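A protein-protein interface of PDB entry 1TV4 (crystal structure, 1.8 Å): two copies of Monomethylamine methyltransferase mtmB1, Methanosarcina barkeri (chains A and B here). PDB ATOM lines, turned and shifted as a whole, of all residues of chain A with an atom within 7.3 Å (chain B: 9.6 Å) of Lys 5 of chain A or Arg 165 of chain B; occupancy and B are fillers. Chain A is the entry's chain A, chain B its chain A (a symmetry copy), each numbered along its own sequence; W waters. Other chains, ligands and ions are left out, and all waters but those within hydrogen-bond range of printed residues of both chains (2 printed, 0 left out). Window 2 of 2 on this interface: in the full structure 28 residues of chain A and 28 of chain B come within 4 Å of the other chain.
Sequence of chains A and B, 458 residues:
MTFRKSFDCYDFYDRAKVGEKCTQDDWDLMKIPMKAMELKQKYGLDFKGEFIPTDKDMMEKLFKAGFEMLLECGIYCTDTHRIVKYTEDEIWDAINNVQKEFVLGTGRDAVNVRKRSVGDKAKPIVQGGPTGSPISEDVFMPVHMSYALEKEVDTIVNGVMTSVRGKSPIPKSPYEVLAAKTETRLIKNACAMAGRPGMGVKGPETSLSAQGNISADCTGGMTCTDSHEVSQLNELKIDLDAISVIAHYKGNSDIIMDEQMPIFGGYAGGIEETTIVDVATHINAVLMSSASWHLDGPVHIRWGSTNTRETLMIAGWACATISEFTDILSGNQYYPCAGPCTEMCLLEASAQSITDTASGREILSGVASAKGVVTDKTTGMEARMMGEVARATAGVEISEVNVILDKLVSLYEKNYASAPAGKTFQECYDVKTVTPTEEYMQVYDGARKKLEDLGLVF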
ATOM      1  N   THR A   2       4.294  11.093  33.486  1.00  0.00           N
ATOM      2  CA  THR A   2       2.839  10.793  33.613  1.00  0.00           C
ATOM      3  C   THR A   2       2.193  10.891  32.237  1.00  0.00           C
ATOM      4  O   THR A   2       2.857  11.232  31.257  1.00  0.00           O
ATOM      5  CB  THR A   2       2.147  11.787  34.576  1.00  0.00           C
ATOM      6  OG1 THR A   2       0.799  11.365  34.813  1.00  0.00           O
ATOM      7  CG2 THR A   2       2.135  13.190  33.983  1.00  0.00           C
ATOM      8  N   PHE A   3       0.900  10.594  32.162  1.00  0.00           N
ATOM      9  CA  PHE A   3       0.180  10.644  30.893  1.00  0.00           C
ATOM     10  C   PHE A   3      -0.421  12.022  30.617  1.00  0.00           C
ATOM     11  O   PHE A   3      -0.629  12.815  31.539  1.00  0.00           O
ATOM     12  CB  PHE A   3      -0.917   9.569  30.887  1.00  0.00           C
ATOM     13  CG  PHE A   3      -1.827   9.621  32.086  1.00  0.00           C
ATOM     14  CD1 PHE A   3      -3.010  10.354  32.052  1.00  0.00           C
ATOM     15  CD2 PHE A   3      -1.493   8.943  33.258  1.00  0.00           C
ATOM     16  CE1 PHE A   3      -3.848  10.411  33.165  1.00  0.00           C
ATOM     17  CE2 PHE A   3      -2.326   8.995  34.381  1.00  0.00           C
ATOM     18  CZ  PHE A   3      -3.507   9.731  34.332  1.00  0.00           C
ATOM     19  N   ARG A   4      -0.676  12.309  29.342  1.00  0.00           N
ATOM     20  CA  ARG A   4      -1.267  13.587  28.939  1.00  0.00           C
ATOM     21  C   ARG A   4      -2.678  13.680  29.499  1.00  0.00           C
ATOM     22  O   ARG A   4      -3.015  14.610  30.232  1.00  0.00           O
ATOM     23  CB  ARG A   4      -1.333  13.687  27.414  1.00  0.00           C
ATOM     24  CG  ARG A   4      -0.019  14.017  26.736  1.00  0.00           C
ATOM     25  CD  ARG A   4       0.292  15.501  26.843  1.00  0.00           C
ATOM     26  NE  ARG A   4       1.508  15.850  26.114  1.00  0.00           N
ATOM     27  CZ  ARG A   4       1.975  17.087  25.983  1.00  0.00           C
ATOM     28  NH1 ARG A   4       1.327  18.107  26.532  1.00  0.00           N
ATOM     29  NH2 ARG A   4       3.092  17.303  25.301  1.00  0.00           N
ATOM     30  N   LYS A   5      -3.494  12.699  29.135  1.00  0.00           N
ATOM     31  CA  LYS A   5      -4.878  12.626  29.582  1.00  0.00           C
ATOM     32  C   LYS A   5      -5.298  11.163  29.572  1.00  0.00           C
ATOM     33  O   LYS A   5      -4.679  10.340  28.892  1.00  0.00           O
ATOM     34  CB  LYS A   5      -5.784  13.428  28.640  1.00  0.00           C
ATOM     35  CG  LYS A   5      -5.760  12.944  27.193  1.00  0.00           C
ATOM     36  CD  LYS A   5      -6.677  13.769  26.288  1.00  0.00           C
ATOM     37  CE  LYS A   5      -8.151  13.507  26.574  1.00  0.00           C
ATOM     38  NZ  LYS A   5      -8.564  12.107  26.254  1.00  0.00           N
ATOM     39  N   SER A   6      -6.335  10.829  30.334  1.00  0.00           N
ATOM     40  CA  SER A   6      -6.809   9.454  30.344  1.00  0.00           C
ATOM     41  C   SER A   6      -7.156   9.127  28.903  1.00  0.00           C
ATOM     42  O   SER A   6      -7.805   9.915  28.215  1.00  0.00           O
ATOM     43  CB  SER A   6      -8.043   9.310  31.235  1.00  0.00           C
ATOM     44  OG  SER A   6      -7.703   9.527  32.593  1.00  0.00           O
ATOM     45  N   PHE A   7      -6.722   7.962  28.445  1.00  0.00           N
ATOM     46  CA  PHE A   7      -6.956   7.552  27.068  1.00  0.00           C
ATOM     47  C   PHE A   7      -8.417   7.240  26.750  1.00  0.00           C
ATOM     48  O   PHE A   7      -9.120   6.620  27.551  1.00  0.00           O
ATOM     49  CB  PHE A   7      -6.105   6.321  26.754  1.00  0.00           C
ATOM     50  CG  PHE A   7      -6.074   5.962  25.297  1.00  0.00           C
ATOM     51  CD1 PHE A   7      -5.119   6.519  24.450  1.00  0.00           C
ATOM     52  CD2 PHE A   7      -7.012   5.084  24.766  1.00  0.00           C
ATOM     53  CE1 PHE A   7      -5.102   6.203  23.091  1.00  0.00           C
ATOM     54  CE2 PHE A   7      -7.005   4.761  23.411  1.00  0.00           C
ATOM     55  CZ  PHE A   7      -6.048   5.322  22.573  1.00  0.00           C
ATOM     56  N   ASP A   8      -8.872   7.684  25.580  1.00  0.00           N
ATOM     57  CA  ASP A   8     -10.231   7.407  25.137  1.00  0.00           C
ATOM     58  C   ASP A   8     -10.276   7.198  23.627  1.00  0.00           C
ATOM     59  O   ASP A   8      -9.257   7.311  22.942  1.00  0.00           O
ATOM     60  CB  ASP A   8     -11.212   8.520  25.556  1.00  0.00           C
ATOM     61  CG  ASP A   8     -10.831   9.887  25.024  1.00  0.00           C
ATOM     62  OD1 ASP A   8     -10.257   9.973  23.919  1.00  0.00           O
ATOM     63  OD2 ASP A   8     -11.136  10.888  25.711  1.00  0.00           O
ATOM     64  N   CYS A   9     -11.461   6.883  23.116  1.00  0.00           N
ATOM     65  CA  CYS A   9     -11.645   6.625  21.693  1.00  0.00           C
ATOM     66  C   CYS A   9     -11.194   7.776  20.800  1.00  0.00           C
ATOM     67  O   CYS A   9     -10.793   7.558  19.656  1.00  0.00           O
ATOM     68  CB  CYS A   9     -13.111   6.284  21.413  1.00  0.00           C
ATOM     69  SG  CYS A   9     -14.277   7.550  21.964  1.00  0.00           S
ATOM     70  N   TYR A  10     -11.253   8.998  21.315  1.00  0.00           N
ATOM     71  CA  TYR A  10     -10.835  10.159  20.536  1.00  0.00           C
ATOM     72  C   TYR A  10      -9.319  10.145  20.357  1.00  0.00           C
ATOM     73  O   TYR A  10      -8.814  10.404  19.265  1.00  0.00           O
ATOM     74  CB  TYR A  10     -11.297  11.446  21.226  1.00  0.00           C
ATOM     75  CG  TYR A  10     -12.795  11.473  21.426  1.00  0.00           C
ATOM     76  CD1 TYR A  10     -13.361  11.153  22.661  1.00  0.00           C
ATOM     77  CD2 TYR A  10     -13.650  11.755  20.360  1.00  0.00           C
ATOM     78  CE1 TYR A  10     -14.745  11.108  22.828  1.00  0.00           C
ATOM     79  CE2 TYR A  10     -15.038  11.712  20.516  1.00  0.00           C
ATOM     80  CZ  TYR A  10     -15.577  11.387  21.748  1.00  0.00           C
ATOM     81  OH  TYR A  10     -16.945  11.318  21.891  1.00  0.00           O
ATOM     82  N   ASP A  11      -8.600   9.833  21.433  1.00  0.00           N
ATOM     83  CA  ASP A  11      -7.145   9.756  21.367  1.00  0.00           C
ATOM     84  C   ASP A  11      -6.766   8.635  20.405  1.00  0.00           C
ATOM     85  O   ASP A  11      -5.785   8.740  19.667  1.00  0.00           O
ATOM     86  CB  ASP A  11      -6.546   9.453  22.743  1.00  0.00           C
ATOM     87  CG  ASP A  11      -6.857  10.525  23.769  1.00  0.00           C
ATOM     88  OD1 ASP A  11      -6.701  11.723  23.446  1.00  0.00           O
ATOM     89  OD2 ASP A  11      -7.245  10.170  24.904  1.00  0.00           O
ATOM     90  N   ASP A  14      -7.032   9.877  16.834  1.00  0.00           N
ATOM     91  CA  ASP A  14      -5.915  10.779  16.585  1.00  0.00           C
ATOM     92  C   ASP A  14      -4.632  10.008  16.287  1.00  0.00           C
ATOM     93  O   ASP A  14      -3.950  10.281  15.301  1.00  0.00           O
ATOM     94  CB  ASP A  14      -5.695  11.695  17.795  1.00  0.00           C
ATOM     95  CG  ASP A  14      -6.802  12.722  17.963  1.00  0.00           C
ATOM     96  OD1 ASP A  14      -6.854  13.368  19.029  1.00  0.00           O
ATOM     97  OD2 ASP A  14      -7.614  12.895  17.029  1.00  0.00           O
ATOM     98  N   ARG A  15      -4.309   9.040  17.138  1.00  0.00           N
ATOM     99  CA  ARG A  15      -3.096   8.249  16.957  1.00  0.00           C
ATOM    100  C   ARG A  15      -3.145   7.317  15.752  1.00  0.00           C
ATOM    101  O   ARG A  15      -2.129   7.096  15.090  1.00  0.00           O
ATOM    102  CB  ARG A  15      -2.807   7.446  18.228  1.00  0.00           C
ATOM    103  CG  ARG A  15      -2.612   8.333  19.441  1.00  0.00           C
ATOM    104  CD  ARG A  15      -2.180   7.555  20.672  1.00  0.00           C
ATOM    105  NE  ARG A  15      -2.194   8.421  21.848  1.00  0.00           N
ATOM    106  CZ  ARG A  15      -1.878   8.034  23.077  1.00  0.00           C
ATOM    107  NH1 ARG A  15      -1.512   6.779  23.311  1.00  0.00           N
ATOM    108  NH2 ARG A  15      -1.948   8.903  24.078  1.00  0.00           N
ATOM    109  N   GLU A  90      -0.504   5.275  30.774  1.00  0.00           N
ATOM    110  CA  GLU A  90      -1.869   5.338  30.263  1.00  0.00           C
ATOM    111  C   GLU A  90      -2.590   4.032  30.571  1.00  0.00           C
ATOM    112  O   GLU A  90      -3.765   4.035  30.944  1.00  0.00           O
ATOM    113  CB  GLU A  90      -1.873   5.583  28.750  1.00  0.00           C
ATOM    114  CG  GLU A  90      -1.229   6.896  28.339  1.00  0.00           C
ATOM    115  CD  GLU A  90      -1.165   7.083  26.834  1.00  0.00           C
ATOM    116  OE1 GLU A  90      -1.130   6.070  26.103  1.00  0.00           O
ATOM    117  OE2 GLU A  90      -1.131   8.248  26.385  1.00  0.00           O
ATOM    118  N   ASP A  93      -3.479   3.869  34.294  1.00  0.00           N
ATOM    119  CA  ASP A  93      -4.557   4.800  34.617  1.00  0.00           C
ATOM    120  C   ASP A  93      -5.895   4.124  34.292  1.00  0.00           C
ATOM    121  O   ASP A  93      -6.867   4.250  35.044  1.00  0.00           O
ATOM    122  CB  ASP A  93      -4.391   6.096  33.815  1.00  0.00           C
ATOM    123  CG  ASP A  93      -5.576   7.041  33.964  1.00  0.00           C
ATOM    124  OD1 ASP A  93      -6.289   7.249  32.961  1.00  0.00           O
ATOM    125  OD2 ASP A  93      -5.789   7.575  35.076  1.00  0.00           O
ATOM    126  N   LYS A 250     -20.669   6.221  24.887  1.00  0.00           N
ATOM    127  CA  LYS A 250     -20.199   7.095  25.963  1.00  0.00           C
ATOM    128  C   LYS A 250     -21.048   8.361  26.041  1.00  0.00           C
ATOM    129  O   LYS A 250     -21.389   8.826  27.131  1.00  0.00           O
ATOM    130  CB  LYS A 250     -18.732   7.484  25.734  1.00  0.00           C
ATOM    131  CG  LYS A 250     -17.735   6.338  25.922  1.00  0.00           C
ATOM    132  CD  LYS A 250     -16.350   6.698  25.374  1.00  0.00           C
ATOM    133  CE  LYS A 250     -15.688   7.848  26.132  1.00  0.00           C
ATOM    134  NZ  LYS A 250     -15.299   7.470  27.524  1.00  0.00           N
ATOM    135  N   SER B 136     -16.950  29.201  15.516  1.00  0.00           N
ATOM    136  CA  SER B 136     -15.821  28.817  16.356  1.00  0.00           C
ATOM    137  C   SER B 136     -16.313  28.168  17.643  1.00  0.00           C
ATOM    138  O   SER B 136     -17.304  28.602  18.233  1.00  0.00           O
ATOM    139  CB  SER B 136     -14.966  30.043  16.693  1.00  0.00           C
ATOM    140  OG  SER B 136     -14.445  30.633  15.513  1.00  0.00           O
ATOM    141  N   GLU B 137     -15.604  27.137  18.083  1.00  0.00           N
ATOM    142  CA  GLU B 137     -15.992  26.423  19.287  1.00  0.00           C
ATOM    143  C   GLU B 137     -16.140  27.306  20.523  1.00  0.00           C
ATOM    144  O   GLU B 137     -17.116  27.167  21.260  1.00  0.00           O
ATOM    145  CB  GLU B 137     -15.001  25.289  19.586  1.00  0.00           C
ATOM    146  CG  GLU B 137     -15.467  24.397  20.740  1.00  0.00           C
ATOM    147  CD  GLU B 137     -14.574  23.198  21.003  1.00  0.00           C
ATOM    148  OE1 GLU B 137     -14.920  22.404  21.910  1.00  0.00           O
ATOM    149  OE2 GLU B 137     -13.537  23.039  20.318  1.00  0.00           O
ATOM    150  N   ASP B 138     -15.201  28.225  20.750  1.00  0.00           N
ATOM    151  CA  ASP B 138     -15.284  29.056  21.951  1.00  0.00           C
ATOM    152  C   ASP B 138     -16.408  30.082  22.014  1.00  0.00           C
ATOM    153  O   ASP B 138     -16.593  30.727  23.048  1.00  0.00           O
ATOM    154  CB  ASP B 138     -13.941  29.740  22.251  1.00  0.00           C
ATOM    155  CG  ASP B 138     -13.477  30.651  21.139  1.00  0.00           C
ATOM    156  OD1 ASP B 138     -14.319  31.146  20.363  1.00  0.00           O
ATOM    157  OD2 ASP B 138     -12.251  30.887  21.059  1.00  0.00           O
ATOM    158  N   MET B 161     -20.223  23.362  14.325  1.00  0.00           N
ATOM    159  CA  MET B 161     -19.041  23.499  15.176  1.00  0.00           C
ATOM    160  C   MET B 161     -17.785  23.324  14.319  1.00  0.00           C
ATOM    161  O   MET B 161     -17.618  22.283  13.686  1.00  0.00           O
ATOM    162  CB  MET B 161     -19.036  22.426  16.277  1.00  0.00           C
ATOM    163  CG  MET B 161     -20.242  22.451  17.220  1.00  0.00           C
ATOM    164  SD  MET B 161     -20.053  21.295  18.618  1.00  0.00           S
ATOM    165  CE  MET B 161     -18.939  22.245  19.681  1.00  0.00           C
ATOM    166  N   THR B 162     -16.907  24.324  14.290  1.00  0.00           N
ATOM    167  CA  THR B 162     -15.679  24.202  13.503  1.00  0.00           C
ATOM    168  C   THR B 162     -14.791  23.152  14.162  1.00  0.00           C
ATOM    169  O   THR B 162     -13.985  22.497  13.499  1.00  0.00           O
ATOM    170  CB  THR B 162     -14.913  25.539  13.406  1.00  0.00           C
ATOM    171  OG1 THR B 162     -14.643  26.035  14.723  1.00  0.00           O
ATOM    172  CG2 THR B 162     -15.732  26.562  12.626  1.00  0.00           C
ATOM    173  N   SER B 163     -14.949  23.006  15.474  1.00  0.00           N
ATOM    174  CA  SER B 163     -14.194  22.030  16.253  1.00  0.00           C
ATOM    175  C   SER B 163     -14.976  21.638  17.499  1.00  0.00           C
ATOM    176  O   SER B 163     -15.893  22.345  17.921  1.00  0.00           O
ATOM    177  CB  SER B 163     -12.844  22.604  16.700  1.00  0.00           C
ATOM    178  OG  SER B 163     -11.990  22.880  15.608  1.00  0.00           O
ATOM    179  N   VAL B 164     -14.616  20.494  18.070  1.00  0.00           N
ATOM    180  CA  VAL B 164     -15.226  20.024  19.307  1.00  0.00           C
ATOM    181  C   VAL B 164     -14.032  19.446  20.061  1.00  0.00           C
ATOM    182  O   VAL B 164     -13.321  18.577  19.550  1.00  0.00           O
ATOM    183  CB  VAL B 164     -16.336  18.966  19.064  1.00  0.00           C
ATOM    184  CG1 VAL B 164     -15.784  17.740  18.356  1.00  0.00           C
ATOM    185  CG2 VAL B 164     -16.974  18.594  20.394  1.00  0.00           C
ATOM    186  N   ARG B 165     -13.795  19.957  21.265  1.00  0.00           N
ATOM    187  CA  ARG B 165     -12.640  19.550  22.055  1.00  0.00           C
ATOM    188  C   ARG B 165     -11.368  19.814  21.245  1.00  0.00           C
ATOM    189  O   ARG B 165     -10.405  19.042  21.277  1.00  0.00           O
ATOM    190  CB  ARG B 165     -12.750  18.079  22.484  1.00  0.00           C
ATOM    191  CG  ARG B 165     -13.496  17.945  23.814  1.00  0.00           C
ATOM    192  CD  ARG B 165     -13.840  16.519  24.184  1.00  0.00           C
ATOM    193  NE  ARG B 165     -12.668  15.662  24.328  1.00  0.00           N
ATOM    194  CZ  ARG B 165     -12.732  14.398  24.733  1.00  0.00           C
ATOM    195  NH1 ARG B 165     -13.909  13.862  25.040  1.00  0.00           N
ATOM    196  NH2 ARG B 165     -11.630  13.668  24.820  1.00  0.00           N
ATOM    197  N   GLY B 166     -11.394  20.922  20.506  1.00  0.00           N
ATOM    198  CA  GLY B 166     -10.252  21.338  19.708  1.00  0.00           C
ATOM    199  C   GLY B 166      -9.914  20.536  18.463  1.00  0.00           C
ATOM    200  O   GLY B 166      -8.840  20.724  17.887  1.00  0.00           O
ATOM    201  N   LYS B 167     -10.816  19.662  18.032  1.00  0.00           N
ATOM    202  CA  LYS B 167     -10.570  18.843  16.849  1.00  0.00           C
ATOM    203  C   LYS B 167     -11.690  18.970  15.823  1.00  0.00           C
ATOM    204  O   LYS B 167     -12.852  19.148  16.185  1.00  0.00           O
ATOM    205  CB  LYS B 167     -10.432  17.374  17.253  1.00  0.00           C
ATOM    206  CG  LYS B 167      -9.253  17.073  18.166  1.00  0.00           C
ATOM    207  CD  LYS B 167      -7.935  17.140  17.409  1.00  0.00           C
ATOM    208  CE  LYS B 167      -6.774  16.742  18.306  1.00  0.00           C
ATOM    209  NZ  LYS B 167      -5.482  16.753  17.569  1.00  0.00           N
ATOM    210  N   SER B 168     -11.339  18.868  14.542  1.00  0.00           N
ATOM    211  CA  SER B 168     -12.332  18.948  13.475  1.00  0.00           C
ATOM    212  C   SER B 168     -13.227  17.721  13.546  1.00  0.00           C
ATOM    213  O   SER B 168     -12.750  16.609  13.741  1.00  0.00           O
ATOM    214  CB  SER B 168     -11.654  18.988  12.102  1.00  0.00           C
ATOM    215  OG  SER B 168     -10.799  20.109  11.988  1.00  0.00           O
ATOM    216  N   PRO B 169     -14.546  17.912  13.393  1.00  0.00           N
ATOM    217  CA  PRO B 169     -15.495  16.796  13.442  1.00  0.00           C
ATOM    218  C   PRO B 169     -15.520  16.027  12.117  1.00  0.00           C
ATOM    219  O   PRO B 169     -16.554  15.934  11.460  1.00  0.00           O
ATOM    220  CB  PRO B 169     -16.815  17.492  13.740  1.00  0.00           C
ATOM    221  CG  PRO B 169     -16.675  18.777  12.978  1.00  0.00           C
ATOM    222  CD  PRO B 169     -15.252  19.203  13.292  1.00  0.00           C
ATOM    223  N   PRO B 174     -14.808   9.631  15.481  1.00  0.00           N
ATOM    224  CA  PRO B 174     -15.616   9.740  16.702  1.00  0.00           C
ATOM    225  C   PRO B 174     -15.957  11.191  17.031  1.00  0.00           C
ATOM    226  O   PRO B 174     -16.927  11.462  17.736  1.00  0.00           O
ATOM    227  CB  PRO B 174     -14.735   9.081  17.766  1.00  0.00           C
ATOM    228  CG  PRO B 174     -13.328   9.311  17.242  1.00  0.00           C
ATOM    229  CD  PRO B 174     -13.494   9.026  15.763  1.00  0.00           C
ATOM    230  N   TYR B 175     -15.160  12.126  16.516  1.00  0.00           N
ATOM    231  CA  TYR B 175     -15.416  13.539  16.766  1.00  0.00           C
ATOM    232  C   TYR B 175     -16.704  13.995  16.089  1.00  0.00           C
ATOM    233  O   TYR B 175     -17.350  14.937  16.546  1.00  0.00           O
ATOM    234  CB  TYR B 175     -14.242  14.398  16.281  1.00  0.00           C
ATOM    235  CG  TYR B 175     -12.991  14.252  17.121  1.00  0.00           C
ATOM    236  CD1 TYR B 175     -11.915  13.476  16.682  1.00  0.00           C
ATOM    237  CD2 TYR B 175     -12.885  14.888  18.357  1.00  0.00           C
ATOM    238  CE1 TYR B 175     -10.759  13.343  17.460  1.00  0.00           C
ATOM    239  CE2 TYR B 175     -11.737  14.761  19.140  1.00  0.00           C
ATOM    240  CZ  TYR B 175     -10.679  13.991  18.684  1.00  0.00           C
ATOM    241  OH  TYR B 175      -9.535  13.888  19.448  1.00  0.00           O
ATOM    242  N   LEU B 178     -19.373  12.971  18.473  1.00  0.00           N
ATOM    243  CA  LEU B 178     -19.315  13.883  19.614  1.00  0.00           C
ATOM    244  C   LEU B 178     -19.969  15.219  19.265  1.00  0.00           C
ATOM    245  O   LEU B 178     -20.742  15.768  20.059  1.00  0.00           O
ATOM    246  CB  LEU B 178     -17.860  14.122  20.044  1.00  0.00           C
ATOM    247  CG  LEU B 178     -17.638  15.072  21.229  1.00  0.00           C
ATOM    248  CD1 LEU B 178     -18.384  14.546  22.455  1.00  0.00           C
ATOM    249  CD2 LEU B 178     -16.142  15.194  21.529  1.00  0.00           C
ATOM    250  N   ALA B 179     -19.665  15.737  18.078  1.00  0.00           N
ATOM    251  CA  ALA B 179     -20.226  17.012  17.638  1.00  0.00           C
ATOM    252  C   ALA B 179     -21.733  16.937  17.407  1.00  0.00           C
ATOM    253  O   ALA B 179     -22.463  17.863  17.756  1.00  0.00           O
ATOM    254  CB  ALA B 179     -19.527  17.486  16.365  1.00  0.00           C
ATOM    255  N   THR B 182     -23.163  16.958  20.946  1.00  0.00           N
ATOM    256  CA  THR B 182     -22.788  18.202  21.621  1.00  0.00           C
ATOM    257  C   THR B 182     -23.461  19.445  21.043  1.00  0.00           C
ATOM    258  O   THR B 182     -23.933  20.314  21.777  1.00  0.00           O
ATOM    259  CB  THR B 182     -21.258  18.383  21.578  1.00  0.00           C
ATOM    260  OG1 THR B 182     -20.636  17.254  22.208  1.00  0.00           O
ATOM    261  CG2 THR B 182     -20.839  19.662  22.302  1.00  0.00           C
ATOM    262  N   LEU B 186     -25.270  22.050  23.597  1.00  0.00           N
ATOM    263  CA  LEU B 186     -24.748  23.391  23.844  1.00  0.00           C
ATOM    264  C   LEU B 186     -25.763  24.463  23.457  1.00  0.00           C
ATOM    265  O   LEU B 186     -25.943  25.452  24.170  1.00  0.00           O
ATOM    266  CB  LEU B 186     -23.454  23.620  23.050  1.00  0.00           C
ATOM    267  CG  LEU B 186     -22.197  22.867  23.494  1.00  0.00           C
ATOM    268  CD1 LEU B 186     -21.039  23.180  22.553  1.00  0.00           C
ATOM    269  CD2 LEU B 186     -21.844  23.275  24.911  1.00  0.00           C
HETATM  270  O   HOH W   1      -9.086  13.210  23.276  1.00  0.00           O
HETATM  271  O   HOH W   2     -14.007  11.119  26.219  1.00  0.00           O
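The side-chain carboxylate of Asp 8 of chain A lies within salt-bridge range of the guanidinium group of Arg 165 of chain B (3.0 Å).
The side-chain amino group (NZ) of Lys 167 of chain B lies within salt-bridge range of the side-chain carboxylate (OD1) of Asp 14 of chain A.
OD1 of Asp 14 of chain A sits at hydrogen-bond distance from OH of Tyr 175 of chain B (2.8 Å).
OD2 of Asp 8 of chain A is in salt-bridge range of NZ of Lys 5 of chain A.
The side-chain amino group of Lys 5 of chain A lies within salt-bridge range of the side-chain carboxylate of Asp 11 of chain A (2.7 Å).
The backbone NH (N) of Tyr 10 of chain A sits at hydrogen-bond distance from the side-chain carboxylate (OD1) of Asp 8 of chain A, at 3.0 Å.
OD1 of Asp 8 of chain A is in hydrogen-bond range of N of Asp 11 of chain A (3.0 Å).
The side-chain carboxylate (OE1) of Glu 137 of chain B lies within hydrogen-bond range of the backbone NH (N) of Arg 165 of chain B, 2.8 Å away.
The backbone carbonyl oxygen (O) of Leu 178 of chain B is in hydrogen-bond range of the side-chain hydroxyl (OG1) of Thr 182 of chain B, 2.6 Å away.
Among the printed residues, pairs that only touch across the chains: Tyr 10 of chain A with Pro 174 of chain B, Tyr 10 of chain A with Leu 178 of chain B, Tyr 10 of chain A with Tyr 175 of chain B, Tyr 10 of chain A with Arg 165 of chain B, Lys 5 of chain A with Arg 165 of chain B and Cys 9 of chain A with Pro 174 of chain B.
Of chain B, only Arg 165 comes within 4 Å of Lys 5 of chain A.
Arg 165 of chain B touches just these residues of chain A: Lys 5 (3.7 Å), Asp 8 (3.0 Å) and Tyr 10 (3.6 Å).
Of the printed residues of chain A, Pro 174 of chain B touches Cys 9 and Tyr 10.
Printed residues of chain A within 4 Å of Tyr 175 of chain B: Tyr 10 (3.5 Å) and Asp 14 (2.8 Å).
Of the printed residues of chain B, Cys 9 of chain A touches Pro 174.
Of the printed residues of chain B, Asp 8 of chain A touches Arg 165 (3.0 Å).
Ser 136 of chain B touches none of the printed residues of chain A.
Thr 162 of chain B touches none of the printed residues of chain A.
Printed residues of chain A that touch a printed residue of chain B: Lys 5, Asp 8, Cys 9, Tyr 10 and Asp 14.
Hydrophobic or aromatic side chains of chain A that line the printed part of chain B: Tyr 10.
Printed residues of chain B that touch a printed residue of chain A: Arg 165, Lys 167, Pro 174, Tyr 175 and Leu 178.
No position is printed for both chains.
Of the 9 pairs that touch across the chains among the printed residues, none has its exchanged pair printed and touching as well.
Water W1 lies within hydrogen-bond range of OD1 of Asp 11 of chain A (2.8 Å), NH2 of Arg 165 of chain B (3.0 Å) and NZ of Lys 5 of chain A (3.2 Å).
Water W2 lies within hydrogen-bond range of OD2 of Asp 8 of chain A (2.9 Å) and NH1 of Arg 165 of chain B (3.0 Å).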
